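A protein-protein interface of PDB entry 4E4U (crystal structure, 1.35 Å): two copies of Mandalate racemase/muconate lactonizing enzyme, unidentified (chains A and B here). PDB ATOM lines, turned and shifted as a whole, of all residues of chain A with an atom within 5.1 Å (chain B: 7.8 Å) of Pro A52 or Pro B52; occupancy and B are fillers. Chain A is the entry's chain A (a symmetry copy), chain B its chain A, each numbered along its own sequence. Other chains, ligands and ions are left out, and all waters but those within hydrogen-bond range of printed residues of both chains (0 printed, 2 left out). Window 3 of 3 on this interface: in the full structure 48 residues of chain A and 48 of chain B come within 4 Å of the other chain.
Pro A52 touches just these residues of chain B: Ala B49 (3.95 Å) and Pro B52 (3.5 Å).
Of the printed residues of chain A, Pro B52 touches Ala A49 (3.95 Å) and Pro A52 (3.5 Å).
No residue of chain B comes within 4 Å of Ala A51.
Printed residues of chain A within 4 Å of Ile B53: Ala A49 (3.9 Å) and Ile A53 (3.6 Å).
Printed residues of chain B within 4 Å of Ile A53: Phe B45 (3.6 Å), Ala B49 (3.9 Å) and Ile B53 (3.6 Å).
Of the printed residues of chain A, Gly B46 touches Asp A56 (3.0 Å).
Printed residues of chain A within 4 Å of Ala B49: Pro A52 and Ile A53.
The nearest residue of chain B that does not touch Pro A52 is Lys B48 (4.2 Å).
The nearest printed residue of chain A that does not touch Ile B53 is Met A50 (6.1 Å).
Of the 17 printed residues of chain B, 5 touch a printed residue of chain A.
Printed residues of chain B that touch a printed residue of chain A: Phe B45, Gly B46, Ala B49, Pro B52 and Ile B53.
Hydrophobic or aromatic side chains of chain A within 4 Å of the printed part of chain B: Ala A49, Pro A52 and Ile A53.
Among the printed residues, 9 pairs touch across the chains.
Among the printed residues, no Asp or Glu carboxylate lies within 4 Å of a Lys or Arg side-chain nitrogen of the other chain.
Ala A49 touches Pro B52, and with the chains exchanged Pro A52 touches Ala B49.
Ala A49 touches Ile B53, and with the chains exchanged Ile A53 touches Ala B49.
Pro B52 touches its own counterpart, Pro A52.
Ile B53 touches its own counterpart, Ile A53.
10 positions are printed for both chains.
Of the 9 pairs that touch across the chains among the printed residues, 6 have their exchanged pair printed and touching as well.
The backbone NH of Gly B46 lies within hydrogen-bond range of the side-chain carboxylate of Asp A56 (3.0 Å).
Ala A49 touches Pro B52.
Ala A49 touches Ile B53.
Ala B49 touches Pro A52 (CB to O, 3.95 Å).
Pro A52 touches Pro B52 (CG to CG, 3.5 Å).
CG2 of Ile A53 touches CE1 of Phe B45 (3.6 Å).
Ala B49 touches Ile A53 (CB to CA, 3.9 Å).
Ile A53 touches Ile B53 (CD1 to CD1, 3.6 Å).
Phe B45 touches Asp A56 (CA to OD2, 3.5 Å).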
ATOM      1  N   PRO A  47     -26.537  -9.537  -4.431  1.00  0.00           N
ATOM      2  CA  PRO A  47     -25.255  -8.834  -4.323  1.00  0.00           C
ATOM      3  C   PRO A  47     -25.364  -7.317  -4.108  1.00  0.00           C
ATOM      4  O   PRO A  47     -24.448  -6.744  -3.518  1.00  0.00           O
ATOM      5  CB  PRO A  47     -24.560  -9.166  -5.653  1.00  0.00           C
ATOM      6  CG  PRO A  47     -25.666  -9.648  -6.567  1.00  0.00           C
ATOM      7  CD  PRO A  47     -26.621 -10.345  -5.658  1.00  0.00           C
ATOM      8  N   LYS A  48     -26.447  -6.681  -4.555  1.00  0.00           N
ATOM      9  CA  LYS A  48     -26.641  -5.248  -4.312  1.00  0.00           C
ATOM     10  C   LYS A  48     -26.832  -4.948  -2.826  1.00  0.00           C
ATOM     11  O   LYS A  48     -26.453  -3.884  -2.332  1.00  0.00           O
ATOM     12  CB  LYS A  48     -27.836  -4.734  -5.109  1.00  0.00           C
ATOM     13  CG  LYS A  48     -27.895  -3.231  -5.275  1.00  0.00           C
ATOM     14  CD  LYS A  48     -28.644  -2.870  -6.552  1.00  0.00           C
ATOM     15  CE  LYS A  48     -28.477  -3.969  -7.604  1.00  0.00           C
ATOM     16  NZ  LYS A  48     -28.422  -3.455  -9.001  1.00  0.00           N
ATOM     17  N   ALA A  49     -27.424  -5.888  -2.109  1.00  0.00           N
ATOM     18  CA  ALA A  49     -27.560  -5.757  -0.668  1.00  0.00           C
ATOM     19  C   ALA A  49     -26.297  -6.236   0.045  1.00  0.00           C
ATOM     20  O   ALA A  49     -25.926  -5.692   1.085  1.00  0.00           O
ATOM     21  CB  ALA A  49     -28.770  -6.533  -0.180  1.00  0.00           C
ATOM     22  N   MET A  50     -25.633  -7.250  -0.508  1.00  0.00           N
ATOM     23  CA  MET A  50     -24.464  -7.821   0.157  1.00  0.00           C
ATOM     24  C   MET A  50     -23.314  -6.825   0.299  1.00  0.00           C
ATOM     25  O   MET A  50     -22.617  -6.834   1.304  1.00  0.00           O
ATOM     26  CB  MET A  50     -23.992  -9.095  -0.550  1.00  0.00           C
ATOM     27  CG  MET A  50     -24.937 -10.279  -0.353  1.00  0.00           C
ATOM     28  SD  MET A  50     -25.165 -10.739   1.372  1.00  0.00           S
ATOM     29  CE  MET A  50     -23.556 -11.417   1.758  1.00  0.00           C
ATOM     30  N   ALA A  51     -23.117  -5.964  -0.693  1.00  0.00           N
ATOM     31  CA  ALA A  51     -22.020  -5.000  -0.615  1.00  0.00           C
ATOM     32  C   ALA A  51     -22.115  -4.067   0.617  1.00  0.00           C
ATOM     33  O   ALA A  51     -21.162  -3.990   1.397  1.00  0.00           O
ATOM     34  CB  ALA A  51     -21.865  -4.225  -1.933  1.00  0.00           C
ATOM     35  N   PRO A  52     -23.267  -3.393   0.833  1.00  0.00           N
ATOM     36  CA  PRO A  52     -23.332  -2.581   2.056  1.00  0.00           C
ATOM     37  C   PRO A  52     -23.393  -3.406   3.346  1.00  0.00           C
ATOM     38  O   PRO A  52     -22.944  -2.921   4.384  1.00  0.00           O
ATOM     39  CB  PRO A  52     -24.615  -1.755   1.873  1.00  0.00           C
ATOM     40  CG  PRO A  52     -25.403  -2.483   0.847  1.00  0.00           C
ATOM     41  CD  PRO A  52     -24.405  -3.118  -0.063  1.00  0.00           C
ATOM     42  N   ILE A  53     -23.916  -4.628   3.296  1.00  0.00           N
ATOM     43  CA  ILE A  53     -23.870  -5.489   4.474  1.00  0.00           C
ATOM     44  C   ILE A  53     -22.417  -5.737   4.890  1.00  0.00           C
ATOM     45  O   ILE A  53     -22.054  -5.610   6.070  1.00  0.00           O
ATOM     46  CB  ILE A  53     -24.545  -6.844   4.200  1.00  0.00           C
ATOM     47  CG1 ILE A  53     -26.066  -6.680   4.130  1.00  0.00           C
ATOM     48  CG2 ILE A  53     -24.190  -7.853   5.282  1.00  0.00           C
ATOM     49  CD1 ILE A  53     -26.775  -7.929   3.670  1.00  0.00           C
ATOM     50  N   ILE A  54     -21.581  -6.082   3.915  1.00  0.00           N
ATOM     51  CA  ILE A  54     -20.188  -6.400   4.203  1.00  0.00           C
ATOM     52  C   ILE A  54     -19.460  -5.183   4.772  1.00  0.00           C
ATOM     53  O   ILE A  54     -18.710  -5.301   5.750  1.00  0.00           O
ATOM     54  CB  ILE A  54     -19.476  -6.931   2.952  1.00  0.00           C
ATOM     55  CG1 ILE A  54     -20.068  -8.286   2.549  1.00  0.00           C
ATOM     56  CG2 ILE A  54     -17.982  -7.064   3.190  1.00  0.00           C
ATOM     57  CD1 ILE A  54     -19.783  -8.666   1.107  1.00  0.00           C
ATOM     58  N   ASP A  55     -19.704  -4.010   4.192  1.00  0.00           N
ATOM     59  CA  ASP A  55     -19.119  -2.775   4.715  1.00  0.00           C
ATOM     60  C   ASP A  55     -19.521  -2.572   6.179  1.00  0.00           C
ATOM     61  O   ASP A  55     -18.697  -2.202   7.017  1.00  0.00           O
ATOM     62  CB  ASP A  55     -19.574  -1.563   3.892  1.00  0.00           C
ATOM     63  CG  ASP A  55     -18.816  -1.410   2.589  1.00  0.00           C
ATOM     64  OD1 ASP A  55     -17.779  -2.079   2.406  1.00  0.00           O
ATOM     65  OD2 ASP A  55     -19.265  -0.600   1.752  1.00  0.00           O
ATOM     66  N   ASP A  56     -20.789  -2.822   6.482  1.00  0.00           N
ATOM     67  CA  ASP A  56     -21.300  -2.608   7.826  1.00  0.00           C
ATOM     68  C   ASP A  56     -20.628  -3.529   8.843  1.00  0.00           C
ATOM     69  O   ASP A  56     -20.188  -3.083   9.906  1.00  0.00           O
ATOM     70  CB  ASP A  56     -22.814  -2.812   7.842  1.00  0.00           C
ATOM     71  CG  ASP A  56     -23.443  -2.394   9.153  1.00  0.00           C
ATOM     72  OD1 ASP A  56     -23.584  -1.170   9.369  1.00  0.00           O
ATOM     73  OD2 ASP A  56     -23.801  -3.279   9.959  1.00  0.00           O
ATOM     74  N   THR B   8     -39.526   2.731   2.258  1.00  0.00           N
ATOM     75  CA  THR B   8     -38.907   2.422   3.541  1.00  0.00           C
ATOM     76  C   THR B   8     -38.588   3.714   4.278  1.00  0.00           C
ATOM     77  O   THR B   8     -38.024   4.643   3.697  1.00  0.00           O
ATOM     78  CB  THR B   8     -37.617   1.619   3.343  1.00  0.00           C
ATOM     79  OG1 THR B   8     -37.940   0.370   2.725  1.00  0.00           O
ATOM     80  CG2 THR B   8     -36.921   1.364   4.677  1.00  0.00           C
ATOM     81  N   ILE B  10     -36.754   4.826   7.804  1.00  0.00           N
ATOM     82  CA  ILE B  10     -36.007   4.477   9.005  1.00  0.00           C
ATOM     83  C   ILE B  10     -35.881   5.729   9.863  1.00  0.00           C
ATOM     84  O   ILE B  10     -35.101   6.636   9.565  1.00  0.00           O
ATOM     85  CB  ILE B  10     -34.635   3.845   8.678  1.00  0.00           C
ATOM     86  CG1 ILE B  10     -34.841   2.569   7.852  1.00  0.00           C
ATOM     87  CG2 ILE B  10     -33.875   3.539   9.966  1.00  0.00           C
ATOM     88  CD1 ILE B  10     -33.564   1.844   7.464  1.00  0.00           C
ATOM     89  N   PHE B  45     -27.447  -5.976  11.200  1.00  0.00           N
ATOM     90  CA  PHE B  45     -26.772  -4.988  10.362  1.00  0.00           C
ATOM     91  C   PHE B  45     -27.450  -3.647  10.552  1.00  0.00           C
ATOM     92  O   PHE B  45     -28.645  -3.599  10.854  1.00  0.00           O
ATOM     93  CB  PHE B  45     -26.848  -5.376   8.881  1.00  0.00           C
ATOM     94  CG  PHE B  45     -26.547  -6.818   8.624  1.00  0.00           C
ATOM     95  CD1 PHE B  45     -25.290  -7.337   8.909  1.00  0.00           C
ATOM     96  CD2 PHE B  45     -27.519  -7.665   8.109  1.00  0.00           C
ATOM     97  CE1 PHE B  45     -25.010  -8.682   8.683  1.00  0.00           C
ATOM     98  CE2 PHE B  45     -27.244  -9.008   7.887  1.00  0.00           C
ATOM     99  CZ  PHE B  45     -25.984  -9.518   8.173  1.00  0.00           C
ATOM    100  N   GLY B  46     -26.693  -2.567  10.354  1.00  0.00           N
ATOM    101  CA  GLY B  46     -27.198  -1.214  10.518  1.00  0.00           C
ATOM    102  C   GLY B  46     -28.146  -0.754   9.427  1.00  0.00           C
ATOM    103  O   GLY B  46     -28.299  -1.421   8.405  1.00  0.00           O
ATOM    104  N   PRO B  47     -28.808   0.382   9.650  1.00  0.00           N
ATOM    105  CA  PRO B  47     -29.824   0.897   8.727  1.00  0.00           C
ATOM    106  C   PRO B  47     -29.322   1.184   7.305  1.00  0.00           C
ATOM    107  O   PRO B  47     -30.128   1.117   6.377  1.00  0.00           O
ATOM    108  CB  PRO B  47     -30.313   2.178   9.422  1.00  0.00           C
ATOM    109  CG  PRO B  47     -29.239   2.511  10.436  1.00  0.00           C
ATOM    110  CD  PRO B  47     -28.726   1.184  10.882  1.00  0.00           C
ATOM    111  N   LYS B  48     -28.036   1.483   7.126  1.00  0.00           N
ATOM    112  CA  LYS B  48     -27.483   1.693   5.784  1.00  0.00           C
ATOM    113  C   LYS B  48     -27.507   0.408   4.957  1.00  0.00           C
ATOM    114  O   LYS B  48     -27.648   0.435   3.733  1.00  0.00           O
ATOM    115  CB  LYS B  48     -26.058   2.230   5.876  1.00  0.00           C
ATOM    116  CG  LYS B  48     -25.532   2.870   4.609  1.00  0.00           C
ATOM    117  CD  LYS B  48     -24.477   3.916   4.945  1.00  0.00           C
ATOM    118  CE  LYS B  48     -24.749   4.535   6.317  1.00  0.00           C
ATOM    119  NZ  LYS B  48     -24.378   5.975   6.406  1.00  0.00           N
ATOM    120  N   ALA B  49     -27.366  -0.724   5.626  1.00  0.00           N
ATOM    121  CA  ALA B  49     -27.483  -2.009   4.958  1.00  0.00           C
ATOM    122  C   ALA B  49     -28.944  -2.440   4.854  1.00  0.00           C
ATOM    123  O   ALA B  49     -29.335  -3.080   3.878  1.00  0.00           O
ATOM    124  CB  ALA B  49     -26.670  -3.060   5.693  1.00  0.00           C
ATOM    125  N   MET B  50     -29.753  -2.093   5.854  1.00  0.00           N
ATOM    126  CA  MET B  50     -31.144  -2.540   5.871  1.00  0.00           C
ATOM    127  C   MET B  50     -31.958  -1.996   4.698  1.00  0.00           C
ATOM    128  O   MET B  50     -32.810  -2.696   4.166  1.00  0.00           O
ATOM    129  CB  MET B  50     -31.820  -2.200   7.202  1.00  0.00           C
ATOM    130  CG  MET B  50     -31.319  -3.051   8.367  1.00  0.00           C
ATOM    131  SD  MET B  50     -31.575  -4.817   8.131  1.00  0.00           S
ATOM    132  CE  MET B  50     -33.356  -4.922   8.270  1.00  0.00           C
ATOM    133  N   ALA B  51     -31.698  -0.761   4.286  1.00  0.00           N
ATOM    134  CA  ALA B  51     -32.459  -0.185   3.178  1.00  0.00           C
ATOM    135  C   ALA B  51     -32.339  -1.001   1.867  1.00  0.00           C
ATOM    136  O   ALA B  51     -33.362  -1.395   1.300  1.00  0.00           O
ATOM    137  CB  ALA B  51     -32.121   1.301   2.982  1.00  0.00           C
ATOM    138  N   PRO B  52     -31.106  -1.302   1.402  1.00  0.00           N
ATOM    139  CA  PRO B  52     -31.046  -2.142   0.198  1.00  0.00           C
ATOM    140  C   PRO B  52     -31.482  -3.594   0.430  1.00  0.00           C
ATOM    141  O   PRO B  52     -31.964  -4.228  -0.507  1.00  0.00           O
ATOM    142  CB  PRO B  52     -29.569  -2.075  -0.218  1.00  0.00           C
ATOM    143  CG  PRO B  52     -28.843  -1.631   0.999  1.00  0.00           C
ATOM    144  CD  PRO B  52     -29.785  -0.740   1.737  1.00  0.00           C
ATOM    145  N   ILE B  53     -31.339  -4.113   1.647  1.00  0.00           N
ATOM    146  CA  ILE B  53     -31.863  -5.445   1.936  1.00  0.00           C
ATOM    147  C   ILE B  53     -33.377  -5.477   1.708  1.00  0.00           C
ATOM    148  O   ILE B  53     -33.911  -6.384   1.050  1.00  0.00           O
ATOM    149  CB  ILE B  53     -31.572  -5.853   3.391  1.00  0.00           C
ATOM    150  CG1 ILE B  53     -30.087  -6.179   3.569  1.00  0.00           C
ATOM    151  CG2 ILE B  53     -32.410  -7.059   3.790  1.00  0.00           C
ATOM    152  CD1 ILE B  53     -29.697  -6.396   5.009  1.00  0.00           C
ATOM    153  N   ILE B  54     -34.071  -4.477   2.244  1.00  0.00           N
ATOM    154  CA  ILE B  54     -35.523  -4.436   2.142  1.00  0.00           C
ATOM    155  C   ILE B  54     -35.962  -4.322   0.681  1.00  0.00           C
ATOM    156  O   ILE B  54     -36.890  -5.019   0.249  1.00  0.00           O
ATOM    157  CB  ILE B  54     -36.101  -3.287   2.979  1.00  0.00           C
ATOM    158  CG1 ILE B  54     -35.863  -3.556   4.469  1.00  0.00           C
ATOM    159  CG2 ILE B  54     -37.585  -3.110   2.711  1.00  0.00           C
ATOM    160  CD1 ILE B  54     -35.960  -2.311   5.332  1.00  0.00           C
ATOM    161  N   ASP B  55     -35.278  -3.479  -0.088  1.00  0.00           N
ATOM    162  CA  ASP B  55     -35.567  -3.359  -1.517  1.00  0.00           C
ATOM    163  C   ASP B  55     -35.417  -4.719  -2.207  1.00  0.00           C
ATOM    164  O   ASP B  55     -36.245  -5.104  -3.036  1.00  0.00           O
ATOM    165  CB  ASP B  55     -34.627  -2.347  -2.183  1.00  0.00           C
ATOM    166  CG  ASP B  55     -35.038  -0.908  -1.945  1.00  0.00           C
ATOM    167  OD1 ASP B  55     -36.169  -0.667  -1.476  1.00  0.00           O
ATOM    168  OD2 ASP B  55     -34.219  -0.016  -2.248  1.00  0.00           O
ATOM    169  N   ASP B  56     -34.362  -5.444  -1.858  1.00  0.00           N
ATOM    170  CA  ASP B  56     -34.083  -6.724  -2.488  1.00  0.00           C
ATOM    171  C   ASP B  56     -35.180  -7.749  -2.203  1.00  0.00           C
ATOM    172  O   ASP B  56     -35.670  -8.421  -3.114  1.00  0.00           O
ATOM    173  CB  ASP B  56     -32.729  -7.249  -2.017  1.00  0.00           C
ATOM    174  CG  ASP B  56     -32.274  -8.464  -2.794  1.00  0.00           C
ATOM    175  OD1 ASP B  56     -31.827  -8.286  -3.948  1.00  0.00           O
ATOM    176  OD2 ASP B  56     -32.354  -9.589  -2.255  1.00  0.00           O
ATOM    177  N   VAL B  57     -35.572  -7.863  -0.939  1.00  0.00           N
ATOM    178  CA  VAL B  57     -36.600  -8.824  -0.553  1.00  0.00           C
ATOM    179  C   VAL B  57     -37.925  -8.473  -1.226  1.00  0.00           C
ATOM    180  O   VAL B  57     -38.622  -9.339  -1.750  1.00  0.00           O
ATOM    181  CB  VAL B  57     -36.783  -8.852   0.974  1.00  0.00           C
ATOM    182  CG1 VAL B  57     -37.912  -9.803   1.370  1.00  0.00           C
ATOM    183  CG2 VAL B  57     -35.474  -9.255   1.659  1.00  0.00           C
ATOM    184  N   PHE B  58     -38.270  -7.192  -1.201  1.00  0.00           N
ATOM    185  CA  PHE B  58     -39.512  -6.738  -1.806  1.00  0.00           C
ATOM    186  C   PHE B  58     -39.562  -7.055  -3.299  1.00  0.00           C
ATOM    187  O   PHE B  58     -40.539  -7.627  -3.798  1.00  0.00           O
ATOM    188  CB  PHE B  58     -39.694  -5.239  -1.588  1.00  0.00           C
ATOM    189  CG  PHE B  58     -40.872  -4.676  -2.314  1.00  0.00           C
ATOM    190  CD1 PHE B  58     -42.157  -4.909  -1.845  1.00  0.00           C
ATOM    191  CD2 PHE B  58     -40.705  -3.929  -3.471  1.00  0.00           C
ATOM    192  CE1 PHE B  58     -43.257  -4.410  -2.517  1.00  0.00           C
ATOM    193  CE2 PHE B  58     -41.805  -3.421  -4.149  1.00  0.00           C
ATOM    194  CZ  PHE B  58     -43.081  -3.659  -3.669  1.00  0.00           C
ATOM    195  N   GLU B  59     -38.502  -6.700  -4.013  1.00  0.00           N
ATOM    196  CA  GLU B  59     -38.468  -6.920  -5.453  1.00  0.00           C
ATOM    197  C   GLU B  59     -38.593  -8.402  -5.811  1.00  0.00           C
ATOM    198  O   GLU B  59     -39.346  -8.758  -6.718  1.00  0.00           O
ATOM    199  CB  GLU B  59     -37.187  -6.335  -6.049  1.00  0.00           C
ATOM    200  CG  GLU B  59     -37.146  -4.820  -6.031  1.00  0.00           C
ATOM    201  CD  GLU B  59     -35.753  -4.268  -6.271  1.00  0.00           C
ATOM    202  OE1 GLU B  59     -34.816  -5.071  -6.476  1.00  0.00           O
ATOM    203  OE2 GLU B  59     -35.595  -3.030  -6.241  1.00  0.00           O
